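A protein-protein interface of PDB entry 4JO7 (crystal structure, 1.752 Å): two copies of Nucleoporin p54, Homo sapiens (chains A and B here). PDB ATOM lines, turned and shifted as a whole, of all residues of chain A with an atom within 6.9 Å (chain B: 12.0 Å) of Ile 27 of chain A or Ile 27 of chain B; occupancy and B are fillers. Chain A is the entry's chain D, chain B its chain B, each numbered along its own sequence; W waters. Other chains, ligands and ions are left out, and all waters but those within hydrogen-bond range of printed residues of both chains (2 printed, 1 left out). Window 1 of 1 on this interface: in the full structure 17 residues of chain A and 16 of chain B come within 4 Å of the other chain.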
ATOM      1  N   GLY A  22     -11.252  20.720   6.863  1.00  0.00           N
ATOM      2  CA  GLY A  22     -10.969  20.084   8.138  1.00  0.00           C
ATOM      3  C   GLY A  22      -9.495  19.761   8.315  1.00  0.00           C
ATOM      4  O   GLY A  22      -8.943  19.931   9.404  1.00  0.00           O
ATOM      5  N   LEU A  23      -8.849  19.282   7.251  1.00  0.00           N
ATOM      6  CA  LEU A  23      -7.419  19.017   7.303  1.00  0.00           C
ATOM      7  C   LEU A  23      -6.659  20.326   7.489  1.00  0.00           C
ATOM      8  O   LEU A  23      -5.706  20.395   8.256  1.00  0.00           O
ATOM      9  CB  LEU A  23      -6.929  18.331   6.024  1.00  0.00           C
ATOM     10  CG  LEU A  23      -7.277  16.857   5.812  1.00  0.00           C
ATOM     11  CD1 LEU A  23      -6.672  16.385   4.492  1.00  0.00           C
ATOM     12  CD2 LEU A  23      -6.791  15.984   6.955  1.00  0.00           C
ATOM     13  N   SER A  24      -7.090  21.362   6.779  1.00  0.00           N
ATOM     14  CA  SER A  24      -6.420  22.653   6.849  1.00  0.00           C
ATOM     15  C   SER A  24      -6.532  23.222   8.260  1.00  0.00           C
ATOM     16  O   SER A  24      -5.597  23.828   8.777  1.00  0.00           O
ATOM     17  CB  SER A  24      -7.019  23.628   5.834  1.00  0.00           C
ATOM     18  OG  SER A  24      -6.314  24.864   5.855  1.00  0.00           O
ATOM     19  N   HIS A  25      -7.683  23.012   8.893  1.00  0.00           N
ATOM     20  CA  HIS A  25      -7.896  23.479  10.250  1.00  0.00           C
ATOM     21  C   HIS A  25      -6.921  22.833  11.193  1.00  0.00           C
ATOM     22  O   HIS A  25      -6.252  23.520  11.995  1.00  0.00           O
ATOM     23  CB  HIS A  25      -9.323  23.181  10.694  1.00  0.00           C
ATOM     24  CG  HIS A  25      -9.656  23.714  12.068  1.00  0.00           C
ATOM     25  ND1 HIS A  25      -9.359  24.969  12.449  1.00  0.00           N
ATOM     26  CD2 HIS A  25     -10.284  23.110  13.157  1.00  0.00           C
ATOM     27  CE1 HIS A  25      -9.772  25.162  13.715  1.00  0.00           C
ATOM     28  NE2 HIS A  25     -10.338  24.023  14.147  1.00  0.00           N
ATOM     29  N   LEU A  26      -6.825  21.511  11.112  1.00  0.00           N
ATOM     30  CA  LEU A  26      -5.905  20.745  11.938  1.00  0.00           C
ATOM     31  C   LEU A  26      -4.454  21.189  11.776  1.00  0.00           C
ATOM     32  O   LEU A  26      -3.745  21.382  12.767  1.00  0.00           O
ATOM     33  CB  LEU A  26      -6.027  19.254  11.633  1.00  0.00           C
ATOM     34  CG  LEU A  26      -7.325  18.581  12.090  1.00  0.00           C
ATOM     35  CD1 LEU A  26      -7.400  17.156  11.556  1.00  0.00           C
ATOM     36  CD2 LEU A  26      -7.433  18.595  13.608  1.00  0.00           C
ATOM     37  N   ILE A  27      -3.993  21.343  10.541  1.00  0.00           N
ATOM     38  CA  ILE A  27      -2.601  21.712  10.335  1.00  0.00           C
ATOM     39  C   ILE A  27      -2.364  23.179  10.732  1.00  0.00           C
ATOM     40  O   ILE A  27      -1.251  23.550  11.084  1.00  0.00           O
ATOM     41  CB  ILE A  27      -2.120  21.394   8.898  1.00  0.00           C
ATOM     42  CG1 ILE A  27      -0.601  21.182   8.899  1.00  0.00           C
ATOM     43  CG2 ILE A  27      -2.561  22.469   7.932  1.00  0.00           C
ATOM     44  CD1 ILE A  27      -0.032  20.670   7.580  1.00  0.00           C
ATOM     45  N   SER A  28      -3.422  23.989  10.720  1.00  0.00           N
ATOM     46  CA  SER A  28      -3.331  25.373  11.170  1.00  0.00           C
ATOM     47  C   SER A  28      -3.062  25.452  12.661  1.00  0.00           C
ATOM     48  O   SER A  28      -2.367  26.353  13.119  1.00  0.00           O
ATOM     49  CB  SER A  28      -4.607  26.146  10.852  1.00  0.00           C
ATOM     50  OG  SER A  28      -4.716  26.371   9.463  1.00  0.00           O
ATOM     51  N   ILE A  29      -3.616  24.510  13.415  1.00  0.00           N
ATOM     52  CA  ILE A  29      -3.372  24.453  14.854  1.00  0.00           C
ATOM     53  C   ILE A  29      -1.909  24.127  15.107  1.00  0.00           C
ATOM     54  O   ILE A  29      -1.263  24.706  15.984  1.00  0.00           O
ATOM     55  CB  ILE A  29      -4.288  23.413  15.527  1.00  0.00           C
ATOM     56  CG1 ILE A  29      -5.745  23.872  15.418  1.00  0.00           C
ATOM     57  CG2 ILE A  29      -3.893  23.213  16.997  1.00  0.00           C
ATOM     58  CD1 ILE A  29      -6.773  22.851  15.876  1.00  0.00           C
ATOM     59  N   ILE A  30      -1.375  23.209  14.314  1.00  0.00           N
ATOM     60  CA  ILE A  30       0.026  22.841  14.414  1.00  0.00           C
ATOM     61  C   ILE A  30       0.890  24.064  14.121  1.00  0.00           C
ATOM     62  O   ILE A  30       1.868  24.336  14.820  1.00  0.00           O
ATOM     63  CB  ILE A  30       0.352  21.675  13.455  1.00  0.00           C
ATOM     64  CG1 ILE A  30      -0.278  20.383  13.984  1.00  0.00           C
ATOM     65  CG2 ILE A  30       1.865  21.506  13.298  1.00  0.00           C
ATOM     66  CD1 ILE A  30      -0.279  19.227  12.996  1.00  0.00           C
ATOM     67  N   LYS A  31       0.524  24.811  13.083  1.00  0.00           N
ATOM     68  CA  LYS A  31       1.241  26.028  12.729  1.00  0.00           C
ATOM     69  C   LYS A  31       1.203  27.039  13.877  1.00  0.00           C
ATOM     70  O   LYS A  31       2.231  27.610  14.258  1.00  0.00           O
ATOM     71  CB  LYS A  31       0.631  26.648  11.474  1.00  0.00           C
ATOM     72  CG  LYS A  31       1.278  27.963  11.035  1.00  0.00           C
ATOM     73  CD  LYS A  31       0.754  28.390   9.671  1.00  0.00           C
ATOM     74  CE  LYS A  31       1.201  29.804   9.302  1.00  0.00           C
ATOM     75  NZ  LYS A  31       0.459  30.843  10.065  1.00  0.00           N
ATOM     76  N   ASP A  32       0.012  27.267  14.415  1.00  0.00           N
ATOM     77  CA  ASP A  32      -0.153  28.185  15.537  1.00  0.00           C
ATOM     78  C   ASP A  32       0.727  27.783  16.725  1.00  0.00           C
ATOM     79  O   ASP A  32       1.317  28.637  17.380  1.00  0.00           O
ATOM     80  CB  ASP A  32      -1.612  28.234  15.991  1.00  0.00           C
ATOM     81  CG  ASP A  32      -2.523  28.921  14.992  1.00  0.00           C
ATOM     82  OD1 ASP A  32      -2.021  29.581  14.052  1.00  0.00           O
ATOM     83  OD2 ASP A  32      -3.760  28.797  15.162  1.00  0.00           O
ATOM     84  N   LEU A  34       3.587  26.086  16.551  1.00  0.00           N
ATOM     85  CA  LEU A  34       4.981  26.343  16.200  1.00  0.00           C
ATOM     86  C   LEU A  34       5.320  27.833  16.248  1.00  0.00           C
ATOM     87  O   LEU A  34       6.471  28.216  16.439  1.00  0.00           O
ATOM     88  CB  LEU A  34       5.291  25.773  14.813  1.00  0.00           C
ATOM     89  CG  LEU A  34       5.418  24.252  14.763  1.00  0.00           C
ATOM     90  CD1 LEU A  34       5.347  23.764  13.310  1.00  0.00           C
ATOM     91  CD2 LEU A  34       6.713  23.801  15.426  1.00  0.00           C
ATOM     92  N   LYS B  17      13.781  29.743  17.097  1.00  0.00           N
ATOM     93  CA  LYS B  17      12.615  30.461  16.593  1.00  0.00           C
ATOM     94  C   LYS B  17      12.625  30.538  15.063  1.00  0.00           C
ATOM     95  O   LYS B  17      11.602  30.337  14.407  1.00  0.00           O
ATOM     96  CB  LYS B  17      12.581  31.869  17.190  1.00  0.00           C
ATOM     97  CG  LYS B  17      11.447  32.747  16.676  1.00  0.00           C
ATOM     98  CD  LYS B  17      10.082  32.196  17.058  1.00  0.00           C
ATOM     99  CE  LYS B  17       8.965  33.119  16.576  1.00  0.00           C
ATOM    100  NZ  LYS B  17       7.619  32.511  16.757  1.00  0.00           N
ATOM    101  N   GLN B  18      13.784  30.824  14.492  1.00  0.00           N
ATOM    102  CA  GLN B  18      13.889  30.893  13.045  1.00  0.00           C
ATOM    103  C   GLN B  18      13.570  29.532  12.414  1.00  0.00           C
ATOM    104  O   GLN B  18      12.982  29.466  11.335  1.00  0.00           O
ATOM    105  CB  GLN B  18      15.277  31.372  12.631  1.00  0.00           C
ATOM    106  CG  GLN B  18      15.399  31.683  11.149  1.00  0.00           C
ATOM    107  CD  GLN B  18      16.610  32.541  10.832  1.00  0.00           C
ATOM    108  OE1 GLN B  18      17.343  32.955  11.729  1.00  0.00           O
ATOM    109  NE2 GLN B  18      16.821  32.816   9.551  1.00  0.00           N
ATOM    110  N   GLN B  19      13.949  28.445  13.083  1.00  0.00           N
ATOM    111  CA  GLN B  19      13.631  27.107  12.576  1.00  0.00           C
ATOM    112  C   GLN B  19      12.141  26.808  12.694  1.00  0.00           C
ATOM    113  O   GLN B  19      11.549  26.177  11.812  1.00  0.00           O
ATOM    114  CB  GLN B  19      14.435  26.044  13.321  1.00  0.00           C
ATOM    115  CG  GLN B  19      15.922  26.246  13.196  1.00  0.00           C
ATOM    116  CD  GLN B  19      16.707  25.270  14.027  1.00  0.00           C
ATOM    117  OE1 GLN B  19      16.157  24.518  14.844  1.00  0.00           O
ATOM    118  NE2 GLN B  19      18.003  25.259  13.815  1.00  0.00           N
ATOM    119  N   GLN B  20      11.529  27.251  13.785  1.00  0.00           N
ATOM    120  CA  GLN B  20      10.086  27.127  13.929  1.00  0.00           C
ATOM    121  C   GLN B  20       9.375  27.841  12.784  1.00  0.00           C
ATOM    122  O   GLN B  20       8.395  27.336  12.238  1.00  0.00           O
ATOM    123  CB  GLN B  20       9.625  27.715  15.262  1.00  0.00           C
ATOM    124  CG  GLN B  20      10.096  26.929  16.476  1.00  0.00           C
ATOM    125  CD  GLN B  20       9.978  27.722  17.762  1.00  0.00           C
ATOM    126  OE1 GLN B  20      10.896  27.730  18.578  1.00  0.00           O
ATOM    127  NE2 GLN B  20       8.848  28.405  17.941  1.00  0.00           N
ATOM    128  N   GLU B  21       9.861  29.028  12.437  1.00  0.00           N
ATOM    129  CA  GLU B  21       9.271  29.812  11.353  1.00  0.00           C
ATOM    130  C   GLU B  21       9.422  29.109  10.005  1.00  0.00           C
ATOM    131  O   GLU B  21       8.550  29.213   9.141  1.00  0.00           O
ATOM    132  CB  GLU B  21       9.894  31.209  11.301  1.00  0.00           C
ATOM    133  CG  GLU B  21       9.515  32.088  12.479  1.00  0.00           C
ATOM    134  CD  GLU B  21      10.329  33.368  12.547  1.00  0.00           C
ATOM    135  OE1 GLU B  21      11.282  33.522  11.752  1.00  0.00           O
ATOM    136  OE2 GLU B  21      10.008  34.224  13.398  1.00  0.00           O
ATOM    137  N   GLY B  22      10.504  28.405   9.812  1.00  0.00           N
ATOM    138  CA  GLY B  22      10.722  27.641   8.618  1.00  0.00           C
ATOM    139  C   GLY B  22       9.670  26.541   8.410  1.00  0.00           C
ATOM    140  O   GLY B  22       9.158  26.334   7.357  1.00  0.00           O
ATOM    141  N   LEU B  23       9.401  25.833   9.489  1.00  0.00           N
ATOM    142  CA  LEU B  23       8.395  24.804   9.474  1.00  0.00           C
ATOM    143  C   LEU B  23       7.058  25.460   9.207  1.00  0.00           C
ATOM    144  O   LEU B  23       6.311  25.010   8.450  1.00  0.00           O
ATOM    145  CB  LEU B  23       8.336  24.054  10.801  1.00  0.00           C
ATOM    146  CG  LEU B  23       9.555  23.224  11.154  1.00  0.00           C
ATOM    147  CD1 LEU B  23       9.467  22.557  12.490  1.00  0.00           C
ATOM    148  CD2 LEU B  23       9.889  22.212  10.113  1.00  0.00           C
ATOM    149  N   SER B  24       6.824  26.553   9.910  1.00  0.00           N
ATOM    150  CA  SER B  24       5.531  27.277   9.623  1.00  0.00           C
ATOM    151  C   SER B  24       5.216  27.770   8.103  1.00  0.00           C
ATOM    152  O   SER B  24       4.210  27.532   7.599  1.00  0.00           O
ATOM    153  CB  SER B  24       5.424  28.490  10.544  1.00  0.00           C
ATOM    154  OG  SER B  24       5.301  28.075  11.894  1.00  0.00           O
ATOM    155  N   HIS B  25       6.313  28.116   7.446  1.00  0.00           N
ATOM    156  CA  HIS B  25       6.276  28.420   6.030  1.00  0.00           C
ATOM    157  C   HIS B  25       5.933  27.201   5.199  1.00  0.00           C
ATOM    158  O   HIS B  25       5.256  27.310   4.235  1.00  0.00           O
ATOM    159  CB  HIS B  25       7.572  29.052   5.546  1.00  0.00           C
ATOM    160  CG  HIS B  25       7.421  29.874   4.293  1.00  0.00           C
ATOM    161  ND1 HIS B  25       6.294  29.890   3.545  1.00  0.00           N
ATOM    162  CD2 HIS B  25       8.308  30.727   3.661  1.00  0.00           C
ATOM    163  CE1 HIS B  25       6.465  30.714   2.528  1.00  0.00           C
ATOM    164  NE2 HIS B  25       7.690  31.231   2.605  1.00  0.00           N
ATOM    165  N   LEU B  26       6.396  26.034   5.594  1.00  0.00           N
ATOM    166  CA  LEU B  26       6.048  24.812   4.870  1.00  0.00           C
ATOM    167  C   LEU B  26       4.548  24.550   5.000  1.00  0.00           C
ATOM    168  O   LEU B  26       3.929  24.193   4.119  1.00  0.00           O
ATOM    169  CB  LEU B  26       6.817  23.612   5.324  1.00  0.00           C
ATOM    170  CG  LEU B  26       8.334  23.644   5.168  1.00  0.00           C
ATOM    171  CD1 LEU B  26       8.982  22.392   5.716  1.00  0.00           C
ATOM    172  CD2 LEU B  26       8.766  23.913   3.734  1.00  0.00           C
ATOM    173  N   ILE B  27       4.044  24.737   6.200  1.00  0.00           N
ATOM    174  CA  ILE B  27       2.645  24.533   6.468  1.00  0.00           C
ATOM    175  C   ILE B  27       1.781  25.454   5.622  1.00  0.00           C
ATOM    176  O   ILE B  27       0.801  25.065   5.111  1.00  0.00           O
ATOM    177  CB  ILE B  27       2.331  24.667   7.969  1.00  0.00           C
ATOM    178  CG1 ILE B  27       2.971  23.513   8.707  1.00  0.00           C
ATOM    179  CG2 ILE B  27       0.850  24.703   8.207  1.00  0.00           C
ATOM    180  CD1 ILE B  27       2.923  23.586  10.195  1.00  0.00           C
ATOM    181  N   SER B  28       2.194  26.700   5.523  1.00  0.00           N
ATOM    182  CA  SER B  28       1.474  27.654   4.705  1.00  0.00           C
ATOM    183  C   SER B  28       1.279  27.147   3.286  1.00  0.00           C
ATOM    184  O   SER B  28       0.269  27.330   2.724  1.00  0.00           O
ATOM    185  CB  SER B  28       2.143  29.041   4.658  1.00  0.00           C
ATOM    186  OG  SER B  28       2.052  29.637   5.875  1.00  0.00           O
ATOM    187  N   ILE B  29       2.295  26.544   2.733  1.00  0.00           N
ATOM    188  CA  ILE B  29       2.211  26.071   1.355  1.00  0.00           C
ATOM    189  C   ILE B  29       1.227  24.906   1.280  1.00  0.00           C
ATOM    190  O   ILE B  29       0.429  24.833   0.358  1.00  0.00           O
ATOM    191  CB  ILE B  29       3.586  25.663   0.794  1.00  0.00           C
ATOM    192  CG1 ILE B  29       4.491  26.891   0.689  1.00  0.00           C
ATOM    193  CG2 ILE B  29       3.436  25.001  -0.592  1.00  0.00           C
ATOM    194  CD1 ILE B  29       5.893  26.578   0.225  1.00  0.00           C
ATOM    195  N   ILE B  30       1.268  24.017   2.270  1.00  0.00           N
ATOM    196  CA  ILE B  30       0.326  22.900   2.335  1.00  0.00           C
ATOM    197  C   ILE B  30      -1.119  23.397   2.446  1.00  0.00           C
ATOM    198  O   ILE B  30      -2.027  22.847   1.820  1.00  0.00           O
ATOM    199  CB  ILE B  30       0.657  21.956   3.514  1.00  0.00           C
ATOM    200  CG1 ILE B  30       1.973  21.224   3.251  1.00  0.00           C
ATOM    201  CG2 ILE B  30      -0.471  20.951   3.734  1.00  0.00           C
ATOM    202  CD1 ILE B  30       2.634  20.679   4.510  1.00  0.00           C
ATOM    203  N   LYS B  31      -1.339  24.432   3.246  1.00  0.00           N
ATOM    204  CA  LYS B  31      -2.678  25.008   3.376  1.00  0.00           C
ATOM    205  C   LYS B  31      -3.161  25.549   2.030  1.00  0.00           C
ATOM    206  O   LYS B  31      -4.320  25.367   1.660  1.00  0.00           O
ATOM    207  CB  LYS B  31      -2.701  26.102   4.446  1.00  0.00           C
ATOM    208  CG  LYS B  31      -2.688  25.552   5.866  1.00  0.00           C
ATOM    209  CD  LYS B  31      -2.601  26.663   6.906  1.00  0.00           C
ATOM    210  CE  LYS B  31      -3.847  27.534   6.893  1.00  0.00           C
ATOM    211  NZ  LYS B  31      -3.832  28.554   7.980  1.00  0.00           N
ATOM    212  N   ASP B  32      -2.264  26.191   1.288  1.00  0.00           N
ATOM    213  CA  ASP B  32      -2.597  26.672  -0.048  1.00  0.00           C
ATOM    214  C   ASP B  32      -2.954  25.510  -0.969  1.00  0.00           C
ATOM    215  O   ASP B  32      -3.931  25.583  -1.713  1.00  0.00           O
ATOM    216  CB  ASP B  32      -1.443  27.473  -0.649  1.00  0.00           C
ATOM    217  CG  ASP B  32      -1.334  28.869  -0.063  1.00  0.00           C
ATOM    218  OD1 ASP B  32      -2.247  29.284   0.679  1.00  0.00           O
ATOM    219  OD2 ASP B  32      -0.340  29.558  -0.359  1.00  0.00           O
ATOM    220  N   ASP B  33      -2.164  24.440  -0.915  1.00  0.00           N
ATOM    221  CA  ASP B  33      -2.479  23.223  -1.660  1.00  0.00           C
ATOM    222  C   ASP B  33      -3.887  22.717  -1.341  1.00  0.00           C
ATOM    223  O   ASP B  33      -4.663  22.409  -2.244  1.00  0.00           O
ATOM    224  CB  ASP B  33      -1.462  22.121  -1.358  1.00  0.00           C
ATOM    225  CG  ASP B  33      -0.072  22.447  -1.864  1.00  0.00           C
ATOM    226  OD1 ASP B  33       0.055  23.269  -2.792  1.00  0.00           O
ATOM    227  OD2 ASP B  33       0.902  21.866  -1.340  1.00  0.00           O
ATOM    228  N   LEU B  34      -4.219  22.636  -0.057  1.00  0.00           N
ATOM    229  CA  LEU B  34      -5.527  22.118   0.359  1.00  0.00           C
ATOM    230  C   LEU B  34      -6.689  23.014  -0.069  1.00  0.00           C
ATOM    231  O   LEU B  34      -7.807  22.540  -0.293  1.00  0.00           O
ATOM    232  CB  LEU B  34      -5.566  21.920   1.875  1.00  0.00           C
ATOM    233  CG  LEU B  34      -4.738  20.750   2.409  1.00  0.00           C
ATOM    234  CD1 LEU B  34      -4.685  20.785   3.914  1.00  0.00           C
ATOM    235  CD2 LEU B  34      -5.307  19.421   1.924  1.00  0.00           C
ATOM    236  N   GLU B  35      -6.435  24.308  -0.167  1.00  0.00           N
ATOM    237  CA  GLU B  35      -7.464  25.245  -0.580  1.00  0.00           C
ATOM    238  C   GLU B  35      -7.711  25.137  -2.083  1.00  0.00           C
ATOM    239  O   GLU B  35      -8.822  25.356  -2.554  1.00  0.00           O
ATOM    240  CB  GLU B  35      -7.060  26.676  -0.209  1.00  0.00           C
ATOM    241  CG  GLU B  35      -7.927  27.757  -0.844  1.00  0.00           C
ATOM    242  CD  GLU B  35      -9.385  27.641  -0.447  1.00  0.00           C
ATOM    243  OE1 GLU B  35      -9.656  27.232   0.702  1.00  0.00           O
ATOM    244  OE2 GLU B  35     -10.261  27.951  -1.283  1.00  0.00           O
ATOM    245  N   ASP B  36      -6.668  24.782  -2.825  1.00  0.00           N
ATOM    246  CA  ASP B  36      -6.705  24.840  -4.283  1.00  0.00           C
ATOM    247  C   ASP B  36      -7.223  23.559  -4.947  1.00  0.00           C
ATOM    248  O   ASP B  36      -7.799  23.619  -6.035  1.00  0.00           O
ATOM    249  CB  ASP B  36      -5.316  25.171  -4.829  1.00  0.00           C
ATOM    250  CG  ASP B  36      -5.316  25.347  -6.331  1.00  0.00           C
ATOM    251  OD1 ASP B  36      -5.943  26.311  -6.809  1.00  0.00           O
ATOM    252  OD2 ASP B  36      -4.692  24.523  -7.032  1.00  0.00           O
HETATM  253  O   HOH W   1      -2.340  28.895  11.119  1.00  0.00           O
HETATM  254  O   HOH W   2      -6.353  25.795   3.328  1.00  0.00           O
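The side-chain amide nitrogen (NE2) of Gln 20 of chain B sits at hydrogen-bond distance from the backbone carbonyl oxygen (O) of Leu 34 of chain A, 2.8 Å away. NZ of Lys 31 of chain B lies within hydrogen-bond range of OG of Ser 28 of chain A (2.8 Å).
CB of Leu 23 of chain A touches CD1 of Leu 34 of chain B (3.9 Å). Lys 31 of chain B touches Ser 24 of chain A. Leu 34 of chain B touches Ser 24 of chain A (CD1 to N, 3.8 Å). Ile 27 of chain B touches Ile 27 of chain A (CG2 to O, 3.7 Å). Ile 27 of chain A touches Lys 31 of chain B. Ile 30 of chain A touches Ile 27 of chain B. Ile 27 of chain B touches Lys 31 of chain A. Lys 31 of chain A touches Ser 28 of chain B (CE to OG, 3.5 Å). Leu 34 of chain A touches Ser 24 of chain B. CD1 of Leu 34 of chain A touches CD1 of Ile 27 of chain B, at 3.95 Å.
Water W2 lies within hydrogen-bond range of the backbone carbonyl oxygen (O) of Lys 31 of chain B (2.7 Å) and the side-chain hydroxyl (OG) of Ser 24 of chain A (2.7 Å). Water W1 lies within hydrogen-bond range of OD1 of Asp 32 of chain A (3.0 Å), O of Ser 28 of chain A (3.2 Å) and NZ of Lys 31 of chain B (3.5 Å).
Leu 23 of chain A touches Leu 34 of chain B, and with the chains exchanged Leu 34 of chain A touches Leu 23 of chain B. Ser 24 of chain A touches Lys 31 of chain B, and with the chains exchanged Lys 31 of chain A touches Ser 24 of chain B. Ile 27 of chain A touches Ile 30 of chain B, and with the chains exchanged Ile 30 of chain A touches Ile 27 of chain B. Ile 27 of chain A touches Lys 31 of chain B, and with the chains exchanged Lys 31 of chain A touches Ile 27 of chain B. Positions printed for both chains: 22, 23, 24, 25, 26, 27, 28, 29, 30, 31, 32 and 34.
Gly 22 of chain A touches none of the printed residues of chain B. Of the printed residues of chain B, Leu 23 of chain A touches Leu 34 (3.9 Å). Ser 24 of chain A touches just these residues of chain B: Lys 31 and Leu 34. No residue of chain B comes within 4 Å of Leu 26 of chain A. Ile 27 of chain A touches three residues of chain B. No residue of chain B comes within 4 Å of Ile 29 of chain A. Of the printed residues of chain B, Ile 30 of chain A touches Ile 27 (3.9 Å). Printed residues of chain B within 4 Å of Leu 34 of chain A: Gln 20, Leu 23, Ser 24 and Ile 27. Ile 27 of chain B touches four residues of chain A. Printed residues of chain A within 4 Å of Ile 30 of chain B: Ile 27. The nearest residue of chain B that does not touch Ile 27 of chain A is Leu 34 of chain B (4.8 Å).
Hydrophobic or aromatic side chains of chain A within 4 Å of the printed part of chain B: Leu 23, Ile 27, Ile 30 and Leu 34. Of the 20 printed residues of chain B, 8 touch a printed residue of chain A. Along chain B the printed residues that touch a printed residue of chain A span positions 20 to 34. Among the printed residues, no Asp or Glu carboxylate lies within 4 Å of a Lys or Arg side-chain nitrogen of the other chain.
The side-chain hydroxyl (OG) of Ser 24 of chain B lies within hydrogen-bond range of the backbone carbonyl oxygen (O) of Gln 20 of chain B (3.2 Å). OG of Ser 28 of chain B lies within hydrogen-bond range of O of Ser 24 of chain B (3.5 Å). The backbone carbonyl oxygen of Ser 24 of chain A is in hydrogen-bond range of the side-chain hydroxyl of Ser 28 of chain A, 2.8 Å away.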
